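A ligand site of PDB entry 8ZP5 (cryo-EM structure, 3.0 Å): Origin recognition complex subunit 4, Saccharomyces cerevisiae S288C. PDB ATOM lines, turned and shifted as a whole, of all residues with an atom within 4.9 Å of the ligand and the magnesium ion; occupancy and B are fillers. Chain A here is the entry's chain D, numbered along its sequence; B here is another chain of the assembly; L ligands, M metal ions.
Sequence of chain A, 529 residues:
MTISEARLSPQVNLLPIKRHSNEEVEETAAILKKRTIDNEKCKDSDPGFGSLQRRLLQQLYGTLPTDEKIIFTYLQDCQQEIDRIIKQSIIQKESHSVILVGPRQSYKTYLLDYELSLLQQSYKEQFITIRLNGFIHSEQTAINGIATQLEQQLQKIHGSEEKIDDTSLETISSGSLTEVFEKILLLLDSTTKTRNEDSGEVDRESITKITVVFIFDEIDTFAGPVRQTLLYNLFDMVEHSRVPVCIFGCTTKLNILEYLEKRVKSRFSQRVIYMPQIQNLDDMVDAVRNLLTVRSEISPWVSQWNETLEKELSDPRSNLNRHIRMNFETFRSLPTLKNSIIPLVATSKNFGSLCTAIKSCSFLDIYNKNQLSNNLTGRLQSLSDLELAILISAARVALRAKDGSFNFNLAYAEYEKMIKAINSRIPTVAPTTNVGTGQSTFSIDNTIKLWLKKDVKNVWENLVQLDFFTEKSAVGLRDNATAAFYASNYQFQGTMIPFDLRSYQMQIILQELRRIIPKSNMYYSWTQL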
ATOM      1  N   TYR A  61      16.077  17.041  -6.463  1.00  0.00           N
ATOM      2  CA  TYR A  61      15.539  18.346  -6.115  1.00  0.00           C
ATOM      3  C   TYR A  61      16.514  19.480  -6.400  1.00  0.00           C
ATOM      4  O   TYR A  61      16.099  20.642  -6.451  1.00  0.00           O
ATOM      5  CB  TYR A  61      15.137  18.379  -4.646  1.00  0.00           C
ATOM      6  CG  TYR A  61      13.783  17.757  -4.373  1.00  0.00           C
ATOM      7  CD1 TYR A  61      12.610  18.415  -4.730  1.00  0.00           C
ATOM      8  CD2 TYR A  61      13.679  16.507  -3.785  1.00  0.00           C
ATOM      9  CE1 TYR A  61      11.378  17.844  -4.485  1.00  0.00           C
ATOM     10  CE2 TYR A  61      12.456  15.932  -3.541  1.00  0.00           C
ATOM     11  CZ  TYR A  61      11.304  16.612  -3.900  1.00  0.00           C
ATOM     12  OH  TYR A  61      10.081  16.037  -3.656  1.00  0.00           O
ATOM     13  N   GLY A  62      17.793  19.166  -6.585  1.00  0.00           N
ATOM     14  CA  GLY A  62      18.781  20.194  -6.880  1.00  0.00           C
ATOM     15  C   GLY A  62      19.219  21.015  -5.695  1.00  0.00           C
ATOM     16  O   GLY A  62      19.789  22.096  -5.882  1.00  0.00           O
ATOM     17  N   LYS A  69      26.752  21.360  -7.772  1.00  0.00           N
ATOM     18  CA  LYS A  69      25.511  21.398  -8.539  1.00  0.00           C
ATOM     19  C   LYS A  69      25.769  20.947  -9.975  1.00  0.00           C
ATOM     20  O   LYS A  69      26.799  21.267 -10.564  1.00  0.00           O
ATOM     21  CB  LYS A  69      24.906  22.798  -8.535  1.00  0.00           C
ATOM     22  CG  LYS A  69      23.988  23.068  -7.350  1.00  0.00           C
ATOM     23  CD  LYS A  69      23.249  24.377  -7.509  1.00  0.00           C
ATOM     24  CE  LYS A  69      22.305  24.624  -6.350  1.00  0.00           C
ATOM     25  NZ  LYS A  69      21.595  25.920  -6.492  1.00  0.00           N
ATOM     26  N   GLY A 102      12.001  31.660 -22.465  1.00  0.00           N
ATOM     27  CA  GLY A 102      11.912  30.214 -22.463  1.00  0.00           C
ATOM     28  C   GLY A 102      10.639  29.739 -21.789  1.00  0.00           C
ATOM     29  O   GLY A 102      10.022  30.459 -20.991  1.00  0.00           O
ATOM     30  N   PRO A 103      10.215  28.520 -22.095  1.00  0.00           N
ATOM     31  CA  PRO A 103       8.963  28.004 -21.534  1.00  0.00           C
ATOM     32  C   PRO A 103       9.026  27.807 -20.027  1.00  0.00           C
ATOM     33  O   PRO A 103      10.065  28.043 -19.416  1.00  0.00           O
ATOM     34  CB  PRO A 103       8.771  26.665 -22.266  1.00  0.00           C
ATOM     35  CG  PRO A 103      10.136  26.270 -22.684  1.00  0.00           C
ATOM     36  CD  PRO A 103      10.862  27.545 -22.996  1.00  0.00           C
ATOM     37  N   ARG A 104       7.905  27.409 -19.425  1.00  0.00           N
ATOM     38  CA  ARG A 104       7.903  27.126 -17.999  1.00  0.00           C
ATOM     39  C   ARG A 104       8.797  25.932 -17.691  1.00  0.00           C
ATOM     40  O   ARG A 104       8.836  24.958 -18.447  1.00  0.00           O
ATOM     41  CB  ARG A 104       6.479  26.853 -17.517  1.00  0.00           C
ATOM     42  CG  ARG A 104       5.579  28.084 -17.512  1.00  0.00           C
ATOM     43  CD  ARG A 104       5.820  28.926 -16.279  1.00  0.00           C
ATOM     44  NE  ARG A 104       5.547  30.338 -16.513  1.00  0.00           N
ATOM     45  CZ  ARG A 104       4.367  30.904 -16.343  1.00  0.00           C
ATOM     46  NH1 ARG A 104       3.311  30.216 -15.950  1.00  0.00           N
ATOM     47  NH2 ARG A 104       4.232  32.207 -16.576  1.00  0.00           N
ATOM     48  N   GLN A 105       9.516  26.015 -16.569  1.00  0.00           N
ATOM     49  CA  GLN A 105      10.460  24.983 -16.148  1.00  0.00           C
ATOM     50  C   GLN A 105      11.515  24.733 -17.222  1.00  0.00           C
ATOM     51  O   GLN A 105      11.854  23.591 -17.553  1.00  0.00           O
ATOM     52  CB  GLN A 105       9.734  23.691 -15.776  1.00  0.00           C
ATOM     53  CG  GLN A 105       8.540  23.907 -14.855  1.00  0.00           C
ATOM     54  CD  GLN A 105       8.954  24.323 -13.461  1.00  0.00           C
ATOM     55  OE1 GLN A 105       9.847  23.739 -12.874  1.00  0.00           O
ATOM     56  NE2 GLN A 105       8.291  25.345 -12.932  1.00  0.00           N
ATOM     57  N   SER A 106      12.051  25.825 -17.778  1.00  0.00           N
ATOM     58  CA  SER A 106      13.137  25.768 -18.746  1.00  0.00           C
ATOM     59  C   SER A 106      14.493  26.076 -18.118  1.00  0.00           C
ATOM     60  O   SER A 106      15.449  26.332 -18.848  1.00  0.00           O
ATOM     61  CB  SER A 106      12.869  26.734 -19.897  1.00  0.00           C
ATOM     62  OG  SER A 106      13.891  26.640 -20.876  1.00  0.00           O
ATOM     63  N   TYR A 107      14.574  26.080 -16.787  1.00  0.00           N
ATOM     64  CA  TYR A 107      15.815  26.329 -16.052  1.00  0.00           C
ATOM     65  C   TYR A 107      16.303  27.770 -16.241  1.00  0.00           C
ATOM     66  O   TYR A 107      17.497  28.010 -16.398  1.00  0.00           O
ATOM     67  CB  TYR A 107      16.900  25.327 -16.428  1.00  0.00           C
ATOM     68  CG  TYR A 107      16.567  23.901 -16.069  1.00  0.00           C
ATOM     69  CD1 TYR A 107      16.796  23.419 -14.795  1.00  0.00           C
ATOM     70  CD2 TYR A 107      16.011  23.044 -17.006  1.00  0.00           C
ATOM     71  CE1 TYR A 107      16.498  22.119 -14.462  1.00  0.00           C
ATOM     72  CE2 TYR A 107      15.707  21.735 -16.682  1.00  0.00           C
ATOM     73  CZ  TYR A 107      15.948  21.280 -15.410  1.00  0.00           C
ATOM     74  OH  TYR A 107      15.642  19.984 -15.076  1.00  0.00           O
ATOM     75  N   LYS A 108      15.370  28.728 -16.229  1.00  0.00           N
ATOM     76  CA  LYS A 108      15.755  30.133 -16.221  1.00  0.00           C
ATOM     77  C   LYS A 108      16.121  30.583 -14.811  1.00  0.00           C
ATOM     78  O   LYS A 108      17.235  31.056 -14.575  1.00  0.00           O
ATOM     79  CB  LYS A 108      14.611  30.996 -16.765  1.00  0.00           C
ATOM     80  CG  LYS A 108      14.214  30.670 -18.192  1.00  0.00           C
ATOM     81  CD  LYS A 108      13.297  31.746 -18.749  1.00  0.00           C
ATOM     82  CE  LYS A 108      11.974  31.753 -18.030  1.00  0.00           C
ATOM     83  NZ  LYS A 108      11.060  30.696 -18.563  1.00  0.00           N
ATOM     84  N   THR A 109      15.187  30.432 -13.873  1.00  0.00           N
ATOM     85  CA  THR A 109      15.471  30.765 -12.481  1.00  0.00           C
ATOM     86  C   THR A 109      16.547  29.848 -11.907  1.00  0.00           C
ATOM     87  O   THR A 109      17.370  30.279 -11.106  1.00  0.00           O
ATOM     88  CB  THR A 109      14.192  30.693 -11.647  1.00  0.00           C
ATOM     89  OG1 THR A 109      13.196  31.526 -12.241  1.00  0.00           O
ATOM     90  CG2 THR A 109      14.459  31.169 -10.233  1.00  0.00           C
ATOM     91  N   TYR A 110      16.556  28.580 -12.324  1.00  0.00           N
ATOM     92  CA  TYR A 110      17.571  27.653 -11.832  1.00  0.00           C
ATOM     93  C   TYR A 110      18.973  28.123 -12.191  1.00  0.00           C
ATOM     94  O   TYR A 110      19.849  28.233 -11.334  1.00  0.00           O
ATOM     95  CB  TYR A 110      17.316  26.247 -12.373  1.00  0.00           C
ATOM     96  CG  TYR A 110      18.412  25.257 -12.053  1.00  0.00           C
ATOM     97  CD1 TYR A 110      18.503  24.683 -10.800  1.00  0.00           C
ATOM     98  CD2 TYR A 110      19.355  24.904 -13.000  1.00  0.00           C
ATOM     99  CE1 TYR A 110      19.497  23.786 -10.488  1.00  0.00           C
ATOM    100  CE2 TYR A 110      20.360  24.011 -12.709  1.00  0.00           C
ATOM    101  CZ  TYR A 110      20.424  23.450 -11.452  1.00  0.00           C
ATOM    102  OH  TYR A 110      21.426  22.549 -11.151  1.00  0.00           O
ATOM    103  N   ASP A 113      19.875  31.534 -10.543  1.00  0.00           N
ATOM    104  CA  ASP A 113      20.191  31.420  -9.122  1.00  0.00           C
ATOM    105  C   ASP A 113      21.480  30.665  -8.882  1.00  0.00           C
ATOM    106  O   ASP A 113      22.216  30.993  -7.946  1.00  0.00           O
ATOM    107  CB  ASP A 113      19.047  30.732  -8.383  1.00  0.00           C
ATOM    108  CG  ASP A 113      17.866  31.647  -8.155  1.00  0.00           C
ATOM    109  OD1 ASP A 113      17.806  32.717  -8.810  1.00  0.00           O
ATOM    110  OD2 ASP A 113      16.991  31.304  -7.335  1.00  0.00           O
ATOM    111  N   ASP A 217      11.533  38.505 -12.756  1.00  0.00           N
ATOM    112  CA  ASP A 217      10.773  37.444 -13.390  1.00  0.00           C
ATOM    113  C   ASP A 217       9.457  37.978 -13.938  1.00  0.00           C
ATOM    114  O   ASP A 217       8.910  38.974 -13.455  1.00  0.00           O
ATOM    115  CB  ASP A 217      10.500  36.314 -12.405  1.00  0.00           C
ATOM    116  CG  ASP A 217      11.765  35.766 -11.769  1.00  0.00           C
ATOM    117  OD1 ASP A 217      12.758  35.571 -12.501  1.00  0.00           O
ATOM    118  OD2 ASP A 217      11.766  35.522 -10.546  1.00  0.00           O
ATOM    119  N   GLU A 218       8.936  37.286 -14.961  1.00  0.00           N
ATOM    120  CA  GLU A 218       7.684  37.636 -15.618  1.00  0.00           C
ATOM    121  C   GLU A 218       7.696  39.097 -16.074  1.00  0.00           C
ATOM    122  O   GLU A 218       6.836  39.900 -15.718  1.00  0.00           O
ATOM    123  CB  GLU A 218       6.490  37.351 -14.713  1.00  0.00           C
ATOM    124  CG  GLU A 218       6.288  35.869 -14.423  1.00  0.00           C
ATOM    125  CD  GLU A 218       5.906  35.084 -15.657  1.00  0.00           C
ATOM    126  OE1 GLU A 218       5.220  35.647 -16.545  1.00  0.00           O
ATOM    127  OE2 GLU A 218       6.276  33.890 -15.740  1.00  0.00           O
ATOM    128  N   THR A 252       8.256  33.920 -20.760  1.00  0.00           N
ATOM    129  CA  THR A 252       7.960  32.798 -21.640  1.00  0.00           C
ATOM    130  C   THR A 252       7.530  33.223 -23.037  1.00  0.00           C
ATOM    131  O   THR A 252       7.489  32.377 -23.934  1.00  0.00           O
ATOM    132  CB  THR A 252       6.873  31.918 -21.029  1.00  0.00           C
ATOM    133  OG1 THR A 252       5.607  32.584 -21.110  1.00  0.00           O
ATOM    134  CG2 THR A 252       7.179  31.634 -19.565  1.00  0.00           C
ATOM    135  N   PRO A 335      11.819  18.175 -15.593  1.00  0.00           N
ATOM    136  CA  PRO A 335      11.059  18.243 -14.327  1.00  0.00           C
ATOM    137  C   PRO A 335       9.961  17.199 -14.208  1.00  0.00           C
ATOM    138  O   PRO A 335       9.745  16.660 -13.114  1.00  0.00           O
ATOM    139  CB  PRO A 335      10.495  19.666 -14.349  1.00  0.00           C
ATOM    140  CG  PRO A 335      11.495  20.432 -15.109  1.00  0.00           C
ATOM    141  CD  PRO A 335      11.990  19.517 -16.181  1.00  0.00           C
ATOM    142  N   LYS A 338      11.711  13.905 -13.327  1.00  0.00           N
ATOM    143  CA  LYS A 338      12.191  13.842 -11.960  1.00  0.00           C
ATOM    144  C   LYS A 338      11.043  13.809 -10.962  1.00  0.00           C
ATOM    145  O   LYS A 338      11.168  13.217  -9.885  1.00  0.00           O
ATOM    146  CB  LYS A 338      13.137  15.011 -11.665  1.00  0.00           C
ATOM    147  CG  LYS A 338      12.482  16.375 -11.574  1.00  0.00           C
ATOM    148  CD  LYS A 338      13.498  17.429 -11.177  1.00  0.00           C
ATOM    149  CE  LYS A 338      14.496  17.670 -12.296  1.00  0.00           C
ATOM    150  NZ  LYS A 338      15.422  18.793 -11.988  1.00  0.00           N
ATOM    151  N   LYS B 151       4.794  31.046  -7.075  1.00  0.00           N
ATOM    152  CA  LYS B 151       6.057  31.766  -7.043  1.00  0.00           C
ATOM    153  C   LYS B 151       6.266  32.549  -5.755  1.00  0.00           C
ATOM    154  O   LYS B 151       7.279  33.230  -5.617  1.00  0.00           O
ATOM    155  CB  LYS B 151       6.153  32.709  -8.244  1.00  0.00           C
ATOM    156  CG  LYS B 151       5.914  32.037  -9.579  1.00  0.00           C
ATOM    157  CD  LYS B 151       7.131  31.256 -10.025  1.00  0.00           C
ATOM    158  CE  LYS B 151       6.764  30.253 -11.108  1.00  0.00           C
ATOM    159  NZ  LYS B 151       7.649  29.044 -11.061  1.00  0.00           N
ATOM    160  N   GLU B 154       9.659  31.956  -3.980  1.00  0.00           N
ATOM    161  CA  GLU B 154      10.933  32.383  -4.553  1.00  0.00           C
ATOM    162  C   GLU B 154      11.479  33.637  -3.881  1.00  0.00           C
ATOM    163  O   GLU B 154      12.683  33.744  -3.655  1.00  0.00           O
ATOM    164  CB  GLU B 154      10.784  32.610  -6.059  1.00  0.00           C
ATOM    165  CG  GLU B 154      10.541  31.346  -6.854  1.00  0.00           C
ATOM    166  CD  GLU B 154      10.341  31.622  -8.333  1.00  0.00           C
ATOM    167  OE1 GLU B 154      10.265  32.809  -8.704  1.00  0.00           O
ATOM    168  OE2 GLU B 154      10.282  30.660  -9.115  1.00  0.00           O
ATOM    169  N   LYS B 158      16.237  32.363   1.001  1.00  0.00           N
ATOM    170  CA  LYS B 158      16.592  30.985   0.729  1.00  0.00           C
ATOM    171  C   LYS B 158      17.301  30.321   1.897  1.00  0.00           C
ATOM    172  O   LYS B 158      17.165  29.112   2.106  1.00  0.00           O
ATOM    173  CB  LYS B 158      17.485  30.910  -0.525  1.00  0.00           C
ATOM    174  CG  LYS B 158      17.719  29.516  -1.053  1.00  0.00           C
ATOM    175  CD  LYS B 158      16.408  28.781  -1.300  1.00  0.00           C
ATOM    176  CE  LYS B 158      16.658  27.368  -1.810  1.00  0.00           C
ATOM    177  NZ  LYS B 158      16.575  27.288  -3.292  1.00  0.00           N
ATOM    178  N   HIS B 182       3.650  24.116 -14.965  1.00  0.00           N
ATOM    179  CA  HIS B 182       4.434  24.428 -13.774  1.00  0.00           C
ATOM    180  C   HIS B 182       5.112  23.215 -13.173  1.00  0.00           C
ATOM    181  O   HIS B 182       5.999  23.375 -12.328  1.00  0.00           O
ATOM    182  CB  HIS B 182       3.550  25.105 -12.727  1.00  0.00           C
ATOM    183  CG  HIS B 182       3.336  26.568 -12.960  1.00  0.00           C
ATOM    184  ND1 HIS B 182       2.124  27.086 -13.351  1.00  0.00           N
ATOM    185  CD2 HIS B 182       4.185  27.614 -12.863  1.00  0.00           C
ATOM    186  CE1 HIS B 182       2.229  28.393 -13.475  1.00  0.00           C
ATOM    187  NE2 HIS B 182       3.470  28.743 -13.185  1.00  0.00           N
HETATM  188  P1  LIG L   1       9.606  29.755 -14.821  1.00  0.00           P
HETATM  189  S1  LIG L   1       9.000  30.740 -16.389  1.00  0.00           S
HETATM  190  O1  LIG L   1      10.509  30.675 -13.953  1.00  0.00           O
HETATM  191  O2  LIG L   1       8.368  29.308 -13.990  1.00  0.00           O
HETATM  192  P2  LIG L   1      11.880  28.253 -14.712  1.00  0.00           P
HETATM  193  O3  LIG L   1      12.875  28.431 -15.790  1.00  0.00           O
HETATM  194  O4  LIG L   1      12.069  29.236 -13.553  1.00  0.00           O
HETATM  195  O5  LIG L   1      10.411  28.494 -15.257  1.00  0.00           O
HETATM  196  P3  LIG L   1      12.995  26.578 -12.856  1.00  0.00           P
HETATM  197  O6  LIG L   1      13.974  27.661 -12.757  1.00  0.00           O
HETATM  198  O7  LIG L   1      12.103  26.429 -11.621  1.00  0.00           O
HETATM  199  O8  LIG L   1      12.007  26.818 -14.063  1.00  0.00           O
HETATM  200  O9  LIG L   1      13.766  25.241 -13.186  1.00  0.00           O
HETATM  201  C1  LIG L   1      13.086  23.978 -13.325  1.00  0.00           C
HETATM  202  C2  LIG L   1      13.593  23.025 -12.268  1.00  0.00           C
HETATM  203  O10 LIG L   1      14.595  23.682 -11.463  1.00  0.00           O
HETATM  204  C3  LIG L   1      12.529  22.505 -11.299  1.00  0.00           C
HETATM  205  O11 LIG L   1      12.713  21.113 -11.053  1.00  0.00           O
HETATM  206  C4  LIG L   1      12.770  23.337 -10.036  1.00  0.00           C
HETATM  207  O12 LIG L   1      12.414  22.627  -8.861  1.00  0.00           O
HETATM  208  C5  LIG L   1      14.285  23.541 -10.096  1.00  0.00           C
HETATM  209  N1  LIG L   1      14.747  24.728  -9.391  1.00  0.00           N
HETATM  210  C6  LIG L   1      14.190  25.981  -9.413  1.00  0.00           C
HETATM  211  N2  LIG L   1      14.831  26.861  -8.680  1.00  0.00           N
HETATM  212  C7  LIG L   1      15.874  26.136  -8.133  1.00  0.00           C
HETATM  213  C8  LIG L   1      16.917  26.490  -7.251  1.00  0.00           C
HETATM  214  N3  LIG L   1      17.082  27.725  -6.757  1.00  0.00           N
HETATM  215  N4  LIG L   1      17.796  25.529  -6.902  1.00  0.00           N
HETATM  216  C9  LIG L   1      17.635  24.304  -7.396  1.00  0.00           C
HETATM  217  N5  LIG L   1      16.695  23.848  -8.222  1.00  0.00           N
HETATM  218  C10 LIG L   1      15.837  24.823  -8.554  1.00  0.00           C
HETATM  219 MG    MG M   1      11.183  31.632 -12.256  1.00  0.00          MG
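An oxygen (O6) of the ligand sits at hydrogen-bond distance from the backbone NH (N) of Thr 109 (3.2 Å).
An oxygen (O2) of the ligand sits at hydrogen-bond distance from the side-chain amino group (NZ) of Lys 151 of chain B (3.0 Å).
An oxygen (O3) of the ligand sits at hydrogen-bond distance from the backbone NH (N) of Lys 108.
An oxygen (O3) of the ligand lies within hydrogen-bond range of the backbone NH (N) of Ser 106, at 3.4 Å.
An oxygen (O3) of the ligand lies within hydrogen-bond range of the backbone NH (N) of Tyr 107, 3.1 Å away.
NE of Arg 104 sits close to S1 of the ligand, at 3.5 Å.
N of Gln 105 lies within hydrogen-bond range of O5 of the ligand (2.9 Å).
The side-chain amino group (NZ) of Lys 108 sits close to a sulfur (S1) of the ligand, 3.0 Å away.
An oxygen (O6) of the ligand lies within hydrogen-bond range of the backbone NH of Tyr 110, 2.8 Å away.
The side-chain amino group of Lys 151 of chain B is in salt-bridge range of the side-chain carboxylate of Glu 154 of chain B (3.7 Å).
The guanidinium group (NH2) of Arg 104 lies within salt-bridge range of the side-chain carboxylate (OE2) of Glu 218, at 2.8 Å.
NE2 of Gln 105 sits at hydrogen-bond distance from O of His 182 of chain B, 3.1 Å away.
The side-chain hydroxyl of Tyr 107 sits at hydrogen-bond distance from the side-chain amino group of Lys 338.
The guanidinium group (NH1) of Arg 104 lies within hydrogen-bond range of a ring nitrogen (NE2) of His 182 of chain B, at 3.1 Å.
O of Pro 103 sits at hydrogen-bond distance from NZ of Lys 108.
O of Gly 102 sits at hydrogen-bond distance from NZ of Lys 108 (2.7 Å).
Tyr 61 touches the ligand.
Gly 62 touches the ligand (O to C9, 3.4 Å).
Lys 69 touches the ligand (NZ to N4, 3.8 Å).
OD2 of Asp 113 touches N3 of the ligand, at 3.6 Å.
CG2 of Thr 252 touches S1 of the ligand, at 3.8 Å.
Lys 338 touches the ligand (NZ to O11, 3.7 Å).
Lys 158 of chain B touches the ligand (NZ to N3, 3.5 Å).
Hydrophobic or aromatic side chains that line the ligand: Tyr 107 and Tyr 110.
Within 4 Å of the ligand: Tyr 61, Gly 62, Lys 69, Arg 104, Gln 105, Ser 106, Tyr 107, Lys 108, Thr 109, Tyr 110, Asp 113, Thr 252, Lys 338, Lys 151 of chain B and Lys 158 of chain B.
Residues that only touch the magnesium ion: Glu 154 of chain B (3.4 Å).
Within 4 Å of the magnesium ion: Thr 109 and Glu 154 of chain B.
The magnesium ion is bound by the side-chain hydroxyl (OG1) of Thr 109 (2.0 Å) and an oxygen (O1) of the ligand (2.1 Å).
The magnesium ion has two donor atoms within binding distance.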
